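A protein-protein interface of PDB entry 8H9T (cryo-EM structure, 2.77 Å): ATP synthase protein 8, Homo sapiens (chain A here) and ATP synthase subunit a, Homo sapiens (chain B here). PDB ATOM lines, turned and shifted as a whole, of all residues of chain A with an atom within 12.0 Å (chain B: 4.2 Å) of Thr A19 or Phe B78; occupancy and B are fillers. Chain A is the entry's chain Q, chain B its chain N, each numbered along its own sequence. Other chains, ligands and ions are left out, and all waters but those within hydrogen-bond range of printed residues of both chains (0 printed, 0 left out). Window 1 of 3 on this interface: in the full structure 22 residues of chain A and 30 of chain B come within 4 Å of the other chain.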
ATOM      1  N   PRO A  10      -4.439 -25.099  -5.430  1.00  0.00           N
ATOM      2  CA  PRO A  10      -5.446 -24.506  -4.534  1.00  0.00           C
ATOM      3  C   PRO A  10      -5.797 -25.367  -3.334  1.00  0.00           C
ATOM      4  O   PRO A  10      -5.883 -24.850  -2.212  1.00  0.00           O
ATOM      5  CB  PRO A  10      -6.648 -24.310  -5.458  1.00  0.00           C
ATOM      6  CG  PRO A  10      -6.045 -24.073  -6.773  1.00  0.00           C
ATOM      7  CD  PRO A  10      -4.848 -24.972  -6.840  1.00  0.00           C
ATOM      8  N   THR A  11      -5.994 -26.670  -3.530  1.00  0.00           N
ATOM      9  CA  THR A  11      -6.353 -27.515  -2.402  1.00  0.00           C
ATOM     10  C   THR A  11      -5.224 -27.674  -1.401  1.00  0.00           C
ATOM     11  O   THR A  11      -5.469 -28.174  -0.301  1.00  0.00           O
ATOM     12  CB  THR A  11      -6.792 -28.894  -2.873  1.00  0.00           C
ATOM     13  OG1 THR A  11      -7.264 -29.645  -1.749  1.00  0.00           O
ATOM     14  CG2 THR A  11      -5.638 -29.624  -3.471  1.00  0.00           C
ATOM     15  N   MET A  12      -4.003 -27.284  -1.747  1.00  0.00           N
ATOM     16  CA  MET A  12      -2.943 -27.204  -0.755  1.00  0.00           C
ATOM     17  C   MET A  12      -2.849 -25.825  -0.132  1.00  0.00           C
ATOM     18  O   MET A  12      -2.509 -25.710   1.047  1.00  0.00           O
ATOM     19  CB  MET A  12      -1.590 -27.559  -1.371  1.00  0.00           C
ATOM     20  CG  MET A  12      -1.499 -28.956  -1.914  1.00  0.00           C
ATOM     21  SD  MET A  12      -1.457 -30.196  -0.626  1.00  0.00           S
ATOM     22  CE  MET A  12      -1.685 -31.668  -1.611  1.00  0.00           C
ATOM     23  N   ILE A  13      -3.145 -24.773  -0.893  1.00  0.00           N
ATOM     24  CA  ILE A  13      -3.041 -23.425  -0.352  1.00  0.00           C
ATOM     25  C   ILE A  13      -4.137 -23.179   0.673  1.00  0.00           C
ATOM     26  O   ILE A  13      -3.858 -22.935   1.850  1.00  0.00           O
ATOM     27  CB  ILE A  13      -3.101 -22.378  -1.473  1.00  0.00           C
ATOM     28  CG1 ILE A  13      -2.085 -22.681  -2.560  1.00  0.00           C
ATOM     29  CG2 ILE A  13      -2.825 -21.012  -0.908  1.00  0.00           C
ATOM     30  CD1 ILE A  13      -0.688 -22.489  -2.128  1.00  0.00           C
ATOM     31  N   THR A  14      -5.399 -23.255   0.248  1.00  0.00           N
ATOM     32  CA  THR A  14      -6.465 -22.672   1.064  1.00  0.00           C
ATOM     33  C   THR A  14      -6.580 -23.271   2.461  1.00  0.00           C
ATOM     34  O   THR A  14      -6.687 -22.493   3.427  1.00  0.00           O
ATOM     35  CB  THR A  14      -7.797 -22.731   0.312  1.00  0.00           C
ATOM     36  OG1 THR A  14      -8.383 -24.027   0.437  1.00  0.00           O
ATOM     37  CG2 THR A  14      -7.588 -22.408  -1.147  1.00  0.00           C
ATOM     38  N   PRO A  15      -6.552 -24.590   2.667  1.00  0.00           N
ATOM     39  CA  PRO A  15      -6.613 -25.071   4.048  1.00  0.00           C
ATOM     40  C   PRO A  15      -5.417 -24.640   4.866  1.00  0.00           C
ATOM     41  O   PRO A  15      -5.537 -24.491   6.086  1.00  0.00           O
ATOM     42  CB  PRO A  15      -6.687 -26.590   3.891  1.00  0.00           C
ATOM     43  CG  PRO A  15      -6.024 -26.847   2.644  1.00  0.00           C
ATOM     44  CD  PRO A  15      -6.368 -25.714   1.738  1.00  0.00           C
ATOM     45  N   MET A  16      -4.269 -24.395   4.240  1.00  0.00           N
ATOM     46  CA  MET A  16      -3.175 -23.800   4.995  1.00  0.00           C
ATOM     47  C   MET A  16      -3.509 -22.381   5.406  1.00  0.00           C
ATOM     48  O   MET A  16      -3.224 -21.979   6.536  1.00  0.00           O
ATOM     49  CB  MET A  16      -1.882 -23.804   4.199  1.00  0.00           C
ATOM     50  CG  MET A  16      -0.698 -23.401   5.040  1.00  0.00           C
ATOM     51  SD  MET A  16      -0.454 -21.635   5.186  1.00  0.00           S
ATOM     52  CE  MET A  16      -0.352 -21.200   3.468  1.00  0.00           C
ATOM     53  N   LEU A  17      -4.062 -21.590   4.490  1.00  0.00           N
ATOM     54  CA  LEU A  17      -4.465 -20.239   4.849  1.00  0.00           C
ATOM     55  C   LEU A  17      -5.361 -20.267   6.073  1.00  0.00           C
ATOM     56  O   LEU A  17      -5.141 -19.525   7.038  1.00  0.00           O
ATOM     57  CB  LEU A  17      -5.175 -19.575   3.677  1.00  0.00           C
ATOM     58  CG  LEU A  17      -4.271 -19.257   2.497  1.00  0.00           C
ATOM     59  CD1 LEU A  17      -4.973 -18.322   1.554  1.00  0.00           C
ATOM     60  CD2 LEU A  17      -2.996 -18.645   2.993  1.00  0.00           C
ATOM     61  N   LEU A  18      -6.350 -21.157   6.069  1.00  0.00           N
ATOM     62  CA  LEU A  18      -7.194 -21.308   7.245  1.00  0.00           C
ATOM     63  C   LEU A  18      -6.357 -21.645   8.468  1.00  0.00           C
ATOM     64  O   LEU A  18      -6.268 -20.854   9.410  1.00  0.00           O
ATOM     65  CB  LEU A  18      -8.246 -22.385   7.015  1.00  0.00           C
ATOM     66  CG  LEU A  18      -9.427 -22.026   6.128  1.00  0.00           C
ATOM     67  CD1 LEU A  18     -10.588 -22.933   6.448  1.00  0.00           C
ATOM     68  CD2 LEU A  18      -9.802 -20.587   6.324  1.00  0.00           C
ATOM     69  N   THR A  19      -5.704 -22.802   8.456  1.00  0.00           N
ATOM     70  CA  THR A  19      -5.095 -23.313   9.674  1.00  0.00           C
ATOM     71  C   THR A  19      -3.933 -22.478  10.175  1.00  0.00           C
ATOM     72  O   THR A  19      -3.493 -22.689  11.306  1.00  0.00           O
ATOM     73  CB  THR A  19      -4.609 -24.730   9.468  1.00  0.00           C
ATOM     74  OG1 THR A  19      -4.168 -25.249  10.720  1.00  0.00           O
ATOM     75  CG2 THR A  19      -3.450 -24.730   8.527  1.00  0.00           C
ATOM     76  N   LEU A  20      -3.416 -21.556   9.380  1.00  0.00           N
ATOM     77  CA  LEU A  20      -2.320 -20.721   9.839  1.00  0.00           C
ATOM     78  C   LEU A  20      -2.761 -19.327  10.215  1.00  0.00           C
ATOM     79  O   LEU A  20      -2.200 -18.744  11.142  1.00  0.00           O
ATOM     80  CB  LEU A  20      -1.237 -20.620   8.767  1.00  0.00           C
ATOM     81  CG  LEU A  20      -0.111 -19.649   9.082  1.00  0.00           C
ATOM     82  CD1 LEU A  20       0.635 -20.119  10.297  1.00  0.00           C
ATOM     83  CD2 LEU A  20       0.815 -19.525   7.912  1.00  0.00           C
ATOM     84  N   PHE A  21      -3.753 -18.773   9.531  1.00  0.00           N
ATOM     85  CA  PHE A  21      -4.183 -17.428   9.845  1.00  0.00           C
ATOM     86  C   PHE A  21      -5.442 -17.388  10.686  1.00  0.00           C
ATOM     87  O   PHE A  21      -5.786 -16.323  11.200  1.00  0.00           O
ATOM     88  CB  PHE A  21      -4.407 -16.638   8.563  1.00  0.00           C
ATOM     89  CG  PHE A  21      -3.146 -16.245   7.884  1.00  0.00           C
ATOM     90  CD1 PHE A  21      -2.788 -14.925   7.785  1.00  0.00           C
ATOM     91  CD2 PHE A  21      -2.314 -17.199   7.345  1.00  0.00           C
ATOM     92  CE1 PHE A  21      -1.630 -14.567   7.161  1.00  0.00           C
ATOM     93  CE2 PHE A  21      -1.153 -16.844   6.719  1.00  0.00           C
ATOM     94  CZ  PHE A  21      -0.811 -15.529   6.624  1.00  0.00           C
ATOM     95  N   LEU A  22      -6.151 -18.501  10.823  1.00  0.00           N
ATOM     96  CA  LEU A  22      -7.358 -18.508  11.635  1.00  0.00           C
ATOM     97  C   LEU A  22      -7.283 -19.495  12.789  1.00  0.00           C
ATOM     98  O   LEU A  22      -7.393 -19.083  13.941  1.00  0.00           O
ATOM     99  CB  LEU A  22      -8.557 -18.805  10.740  1.00  0.00           C
ATOM    100  CG  LEU A  22      -9.923 -18.510  11.323  1.00  0.00           C
ATOM    101  CD1 LEU A  22     -10.819 -18.028  10.214  1.00  0.00           C
ATOM    102  CD2 LEU A  22     -10.492 -19.752  11.963  1.00  0.00           C
ATOM    103  N   ILE A  23      -7.052 -20.777  12.531  1.00  0.00           N
ATOM    104  CA  ILE A  23      -7.286 -21.770  13.573  1.00  0.00           C
ATOM    105  C   ILE A  23      -6.142 -21.806  14.572  1.00  0.00           C
ATOM    106  O   ILE A  23      -6.369 -21.872  15.783  1.00  0.00           O
ATOM    107  CB  ILE A  23      -7.533 -23.146  12.949  1.00  0.00           C
ATOM    108  CG1 ILE A  23      -8.736 -23.082  12.024  1.00  0.00           C
ATOM    109  CG2 ILE A  23      -7.781 -24.155  14.024  1.00  0.00           C
ATOM    110  CD1 ILE A  23      -9.105 -24.401  11.437  1.00  0.00           C
ATOM    111  N   THR A  24      -4.900 -21.778  14.103  1.00  0.00           N
ATOM    112  CA  THR A  24      -3.792 -21.767  15.047  1.00  0.00           C
ATOM    113  C   THR A  24      -3.764 -20.471  15.835  1.00  0.00           C
ATOM    114  O   THR A  24      -3.443 -20.466  17.027  1.00  0.00           O
ATOM    115  CB  THR A  24      -2.472 -21.966  14.325  1.00  0.00           C
ATOM    116  OG1 THR A  24      -2.596 -23.061  13.421  1.00  0.00           O
ATOM    117  CG2 THR A  24      -1.392 -22.276  15.320  1.00  0.00           C
ATOM    118  N   GLN A  25      -4.115 -19.361  15.197  1.00  0.00           N
ATOM    119  CA  GLN A  25      -4.071 -18.097  15.909  1.00  0.00           C
ATOM    120  C   GLN A  25      -5.162 -18.026  16.962  1.00  0.00           C
ATOM    121  O   GLN A  25      -4.951 -17.460  18.036  1.00  0.00           O
ATOM    122  CB  GLN A  25      -4.170 -16.950  14.922  1.00  0.00           C
ATOM    123  CG  GLN A  25      -3.026 -16.965  13.965  1.00  0.00           C
ATOM    124  CD  GLN A  25      -2.836 -15.657  13.273  1.00  0.00           C
ATOM    125  OE1 GLN A  25      -3.616 -14.733  13.450  1.00  0.00           O
ATOM    126  NE2 GLN A  25      -1.783 -15.559  12.483  1.00  0.00           N
ATOM    127  N   LEU A  26      -6.327 -18.604  16.690  1.00  0.00           N
ATOM    128  CA  LEU A  26      -7.330 -18.703  17.740  1.00  0.00           C
ATOM    129  C   LEU A  26      -6.860 -19.628  18.845  1.00  0.00           C
ATOM    130  O   LEU A  26      -7.103 -19.365  20.023  1.00  0.00           O
ATOM    131  CB  LEU A  26      -8.654 -19.196  17.177  1.00  0.00           C
ATOM    132  CG  LEU A  26      -9.310 -18.267  16.175  1.00  0.00           C
ATOM    133  CD1 LEU A  26     -10.688 -18.768  15.847  1.00  0.00           C
ATOM    134  CD2 LEU A  26      -9.355 -16.880  16.729  1.00  0.00           C
ATOM    135  N   LYS A  27      -6.193 -20.722  18.487  1.00  0.00           N
ATOM    136  CA  LYS A  27      -5.679 -21.617  19.514  1.00  0.00           C
ATOM    137  C   LYS A  27      -4.674 -20.910  20.406  1.00  0.00           C
ATOM    138  O   LYS A  27      -4.548 -21.247  21.584  1.00  0.00           O
ATOM    139  CB  LYS A  27      -5.048 -22.847  18.872  1.00  0.00           C
ATOM    140  CG  LYS A  27      -6.048 -23.850  18.349  1.00  0.00           C
ATOM    141  CD  LYS A  27      -6.660 -24.624  19.479  1.00  0.00           C
ATOM    142  CE  LYS A  27      -7.338 -25.875  18.982  1.00  0.00           C
ATOM    143  NZ  LYS A  27      -8.076 -26.562  20.074  1.00  0.00           N
ATOM    144  N   MET A  28      -3.945 -19.939  19.864  1.00  0.00           N
ATOM    145  CA  MET A  28      -3.015 -19.173  20.687  1.00  0.00           C
ATOM    146  C   MET A  28      -3.747 -18.126  21.517  1.00  0.00           C
ATOM    147  O   MET A  28      -3.567 -18.056  22.735  1.00  0.00           O
ATOM    148  CB  MET A  28      -1.963 -18.502  19.816  1.00  0.00           C
ATOM    149  CG  MET A  28      -0.851 -19.385  19.367  1.00  0.00           C
ATOM    150  SD  MET A  28       0.054 -20.053  20.742  1.00  0.00           S
ATOM    151  CE  MET A  28      -0.471 -21.745  20.611  1.00  0.00           C
ATOM    152  N   LEU A  29      -4.586 -17.314  20.873  1.00  0.00           N
ATOM    153  CA  LEU A  29      -5.293 -16.233  21.550  1.00  0.00           C
ATOM    154  C   LEU A  29      -6.021 -16.688  22.798  1.00  0.00           C
ATOM    155  O   LEU A  29      -6.362 -15.855  23.639  1.00  0.00           O
ATOM    156  CB  LEU A  29      -6.296 -15.597  20.603  1.00  0.00           C
ATOM    157  CG  LEU A  29      -5.763 -14.369  19.903  1.00  0.00           C
ATOM    158  CD1 LEU A  29      -6.865 -13.710  19.128  1.00  0.00           C
ATOM    159  CD2 LEU A  29      -5.227 -13.440  20.941  1.00  0.00           C
ATOM    160  N   ILE B  24      -3.872 -30.969   6.555  1.00  0.00           N
ATOM    161  CA  ILE B  24      -3.327 -29.648   6.824  1.00  0.00           C
ATOM    162  C   ILE B  24      -3.976 -29.038   8.055  1.00  0.00           C
ATOM    163  O   ILE B  24      -3.313 -28.365   8.848  1.00  0.00           O
ATOM    164  CB  ILE B  24      -3.487 -28.756   5.586  1.00  0.00           C
ATOM    165  CG1 ILE B  24      -2.485 -29.169   4.516  1.00  0.00           C
ATOM    166  CG2 ILE B  24      -3.285 -27.321   5.945  1.00  0.00           C
ATOM    167  CD1 ILE B  24      -2.668 -28.463   3.211  1.00  0.00           C
ATOM    168  N   LEU B  25      -5.269 -29.279   8.253  1.00  0.00           N
ATOM    169  CA  LEU B  25      -6.010 -28.686   9.360  1.00  0.00           C
ATOM    170  C   LEU B  25      -5.855 -29.442  10.668  1.00  0.00           C
ATOM    171  O   LEU B  25      -6.440 -29.030  11.669  1.00  0.00           O
ATOM    172  CB  LEU B  25      -7.497 -28.598   9.019  1.00  0.00           C
ATOM    173  CG  LEU B  25      -7.888 -27.813   7.774  1.00  0.00           C
ATOM    174  CD1 LEU B  25      -9.353 -27.982   7.496  1.00  0.00           C
ATOM    175  CD2 LEU B  25      -7.563 -26.369   7.965  1.00  0.00           C
ATOM    176  N   PRO B  28      -3.425 -28.057  14.500  1.00  0.00           N
ATOM    177  CA  PRO B  28      -4.054 -27.314  15.601  1.00  0.00           C
ATOM    178  C   PRO B  28      -4.797 -28.188  16.585  1.00  0.00           C
ATOM    179  O   PRO B  28      -4.809 -27.887  17.782  1.00  0.00           O
ATOM    180  CB  PRO B  28      -5.009 -26.368  14.871  1.00  0.00           C
ATOM    181  CG  PRO B  28      -4.353 -26.125  13.619  1.00  0.00           C
ATOM    182  CD  PRO B  28      -3.742 -27.420  13.212  1.00  0.00           C
ATOM    183  N   SER B  74       2.442 -18.388  16.195  1.00  0.00           N
ATOM    184  CA  SER B  74       1.592 -19.348  15.506  1.00  0.00           C
ATOM    185  C   SER B  74       2.299 -19.938  14.305  1.00  0.00           C
ATOM    186  O   SER B  74       2.141 -21.124  14.014  1.00  0.00           O
ATOM    187  CB  SER B  74       0.301 -18.685  15.067  1.00  0.00           C
ATOM    188  OG  SER B  74       0.575 -17.713  14.078  1.00  0.00           O
ATOM    189  N   LEU B  75       3.095 -19.134  13.606  1.00  0.00           N
ATOM    190  CA  LEU B  75       3.860 -19.636  12.477  1.00  0.00           C
ATOM    191  C   LEU B  75       4.811 -20.731  12.910  1.00  0.00           C
ATOM    192  O   LEU B  75       4.829 -21.819  12.325  1.00  0.00           O
ATOM    193  CB  LEU B  75       4.633 -18.496  11.836  1.00  0.00           C
ATOM    194  CG  LEU B  75       5.363 -18.844  10.565  1.00  0.00           C
ATOM    195  CD1 LEU B  75       4.393 -19.502   9.654  1.00  0.00           C
ATOM    196  CD2 LEU B  75       5.872 -17.580   9.950  1.00  0.00           C
ATOM    197  N   ILE B  76       5.617 -20.462  13.932  1.00  0.00           N
ATOM    198  CA  ILE B  76       6.601 -21.458  14.335  1.00  0.00           C
ATOM    199  C   ILE B  76       5.916 -22.702  14.878  1.00  0.00           C
ATOM    200  O   ILE B  76       6.357 -23.823  14.620  1.00  0.00           O
ATOM    201  CB  ILE B  76       7.609 -20.874  15.335  1.00  0.00           C
ATOM    202  CG1 ILE B  76       8.704 -21.885  15.614  1.00  0.00           C
ATOM    203  CG2 ILE B  76       6.959 -20.512  16.616  1.00  0.00           C
ATOM    204  CD1 ILE B  76       9.733 -21.386  16.561  1.00  0.00           C
ATOM    205  N   ILE B  77       4.802 -22.541  15.590  1.00  0.00           N
ATOM    206  CA  ILE B  77       4.120 -23.703  16.147  1.00  0.00           C
ATOM    207  C   ILE B  77       3.531 -24.560  15.037  1.00  0.00           C
ATOM    208  O   ILE B  77       3.666 -25.789  15.040  1.00  0.00           O
ATOM    209  CB  ILE B  77       3.038 -23.262  17.140  1.00  0.00           C
ATOM    210  CG1 ILE B  77       3.670 -22.838  18.456  1.00  0.00           C
ATOM    211  CG2 ILE B  77       2.101 -24.382  17.386  1.00  0.00           C
ATOM    212  CD1 ILE B  77       4.395 -23.951  19.141  1.00  0.00           C
ATOM    213  N   PHE B  78       2.866 -23.927  14.074  1.00  0.00           N
ATOM    214  CA  PHE B  78       2.289 -24.662  12.957  1.00  0.00           C
ATOM    215  C   PHE B  78       3.361 -25.406  12.183  1.00  0.00           C
ATOM    216  O   PHE B  78       3.223 -26.602  11.907  1.00  0.00           O
ATOM    217  CB  PHE B  78       1.545 -23.699  12.044  1.00  0.00           C
ATOM    218  CG  PHE B  78       1.158 -24.283  10.732  1.00  0.00           C
ATOM    219  CD1 PHE B  78       0.219 -25.280  10.661  1.00  0.00           C
ATOM    220  CD2 PHE B  78       1.705 -23.810   9.569  1.00  0.00           C
ATOM    221  CE1 PHE B  78      -0.149 -25.803   9.455  1.00  0.00           C
ATOM    222  CE2 PHE B  78       1.338 -24.333   8.368  1.00  0.00           C
ATOM    223  CZ  PHE B  78       0.412 -25.330   8.312  1.00  0.00           C
ATOM    224  N   ILE B  79       4.446 -24.720  11.829  1.00  0.00           N
ATOM    225  CA  ILE B  79       5.467 -25.375  11.026  1.00  0.00           C
ATOM    226  C   ILE B  79       6.111 -26.510  11.804  1.00  0.00           C
ATOM    227  O   ILE B  79       6.341 -27.592  11.258  1.00  0.00           O
ATOM    228  CB  ILE B  79       6.511 -24.369  10.532  1.00  0.00           C
ATOM    229  CG1 ILE B  79       5.894 -23.422   9.522  1.00  0.00           C
ATOM    230  CG2 ILE B  79       7.612 -25.082   9.842  1.00  0.00           C
ATOM    231  CD1 ILE B  79       6.889 -22.500   8.906  1.00  0.00           C
ATOM    232  N   ALA B  80       6.409 -26.301  13.086  1.00  0.00           N
ATOM    233  CA  ALA B  80       7.079 -27.351  13.838  1.00  0.00           C
ATOM    234  C   ALA B  80       6.186 -28.567  14.012  1.00  0.00           C
ATOM    235  O   ALA B  80       6.654 -29.700  13.885  1.00  0.00           O
ATOM    236  CB  ALA B  80       7.537 -26.827  15.189  1.00  0.00           C
ATOM    237  N   THR B  81       4.898 -28.368  14.292  1.00  0.00           N
ATOM    238  CA  THR B  81       4.028 -29.531  14.414  1.00  0.00           C
ATOM    239  C   THR B  81       3.865 -30.235  13.079  1.00  0.00           C
ATOM    240  O   THR B  81       3.830 -31.465  13.032  1.00  0.00           O
ATOM    241  CB  THR B  81       2.663 -29.151  14.973  1.00  0.00           C
ATOM    242  OG1 THR B  81       2.062 -28.162  14.135  1.00  0.00           O
ATOM    243  CG2 THR B  81       2.791 -28.625  16.378  1.00  0.00           C
ATOM    244  N   THR B  82       3.780 -29.485  11.979  1.00  0.00           N
ATOM    245  CA  THR B  82       3.658 -30.138  10.681  1.00  0.00           C
ATOM    246  C   THR B  82       4.880 -30.996  10.390  1.00  0.00           C
ATOM    247  O   THR B  82       4.758 -32.173  10.032  1.00  0.00           O
ATOM    248  CB  THR B  82       3.458 -29.105   9.581  1.00  0.00           C
ATOM    249  OG1 THR B  82       2.169 -28.514   9.716  1.00  0.00           O
ATOM    250  CG2 THR B  82       3.507 -29.774   8.266  1.00  0.00           C
ATOM    251  N   MET B 104       3.064 -19.582   2.415  1.00  0.00           N
ATOM    252  CA  MET B 104       3.487 -19.121   3.728  1.00  0.00           C
ATOM    253  C   MET B 104       4.569 -18.062   3.645  1.00  0.00           C
ATOM    254  O   MET B 104       4.740 -17.297   4.593  1.00  0.00           O
ATOM    255  CB  MET B 104       4.006 -20.285   4.568  1.00  0.00           C
ATOM    256  CG  MET B 104       2.946 -21.071   5.270  1.00  0.00           C
ATOM    257  SD  MET B 104       3.622 -22.005   6.636  1.00  0.00           S
ATOM    258  CE  MET B 104       4.897 -22.900   5.788  1.00  0.00           C
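The backbone carbonyl oxygen (O) of Leu A18 lies within hydrogen-bond range of the backbone NH (N) of Ile A23 (3.2 Å).
The backbone NH of Thr A24 sits at hydrogen-bond distance from the backbone carbonyl oxygen of Thr A19 (3.3 Å).
The backbone carbonyl oxygen (O) of Leu A20 lies close to the side-chain amide nitrogen (NE2) of Gln A25 (3.5 Å).
The backbone carbonyl oxygen (O) of Phe B78 sits at hydrogen-bond distance from the side-chain hydroxyl (OG1) of Thr B81.
The side-chain hydroxyl (OG1) of Thr B82 is in hydrogen-bond range of the backbone carbonyl oxygen (O) of Phe B78, at 3.1 Å.
Of the printed residues of chain B, Met A12 touches Ile B24 (3.5 Å).
Of chain B, only Ile B24 (3.7 Å), Leu B25 (3.7 Å), Pro B28 (3.0 Å) and Phe B78 (3.6 Å) come within 4 Å of Thr A19.
Of the printed residues of chain B, Thr A24 touches Pro B28 and Ser B74.
Printed residues of chain B within 4 Å of Gln A25: Ser B74.
Printed residues of chain B within 4 Å of Lys A27: Pro B28.
Ser B74 touches just these residues of chain A: Thr A24 and Gln A25.
Leu B75 touches just one residue of chain A: Leu A20.
Phe B78 touches just these residues of chain A: Met A16, Thr A19 and Leu A20.
No residue of chain A comes within 4 Å of Ala B80.
Thr B81 touches none of the printed residues of chain A.
No residue of chain A comes within 4 Å of Thr B82.
Printed residues of chain A within 4 Å of Met B104: Met A16 and Leu A20.
The nearest printed residue of chain B that does not touch Thr A19 is Ser B74 (6.4 Å).
The nearest printed residue of chain B that does not touch Leu A20 is Ser B74 (4.1 Å).
Of the 20 printed residues of chain A, 9 touch a printed residue of chain B.
Printed residues of chain A that touch a printed residue of chain B: Met A12, Pro A15, Met A16, Thr A19, Leu A20, Ile A23, Thr A24, Gln A25 and Lys A27.
Hydrophobic or aromatic side chains of chain A within 4 Å of the printed part of chain B: Pro A15, Met A16, Leu A20 and Ile A23.
Among the printed residues, 18 pairs touch across the chains.
Among the printed residues, no Asp or Glu carboxylate lies within 4 Å of a Lys or Arg side-chain nitrogen of the other chain.
Pro A15 touches Leu B25 (O to CD2, 3.3 Å).
Ile B24 touches Thr A19 (O to CG2, 3.7 Å).
Thr A19 touches Leu B25 (CB to CD2, 3.7 Å).
Leu B75 touches Leu A20 (CD1 to CD1, 3.9 Å).
Phe B78 touches Leu A20.
CG of Met B104 touches CD2 of Leu A20, 3.7 Å away.
Ile A23 touches Pro B28.
Thr A24 touches Ser B74.
Gln A25 touches Ser B74 (NE2 to OG, 3.6 Å).
Lys A27 touches Pro B28 (CE to O, 3.4 Å).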
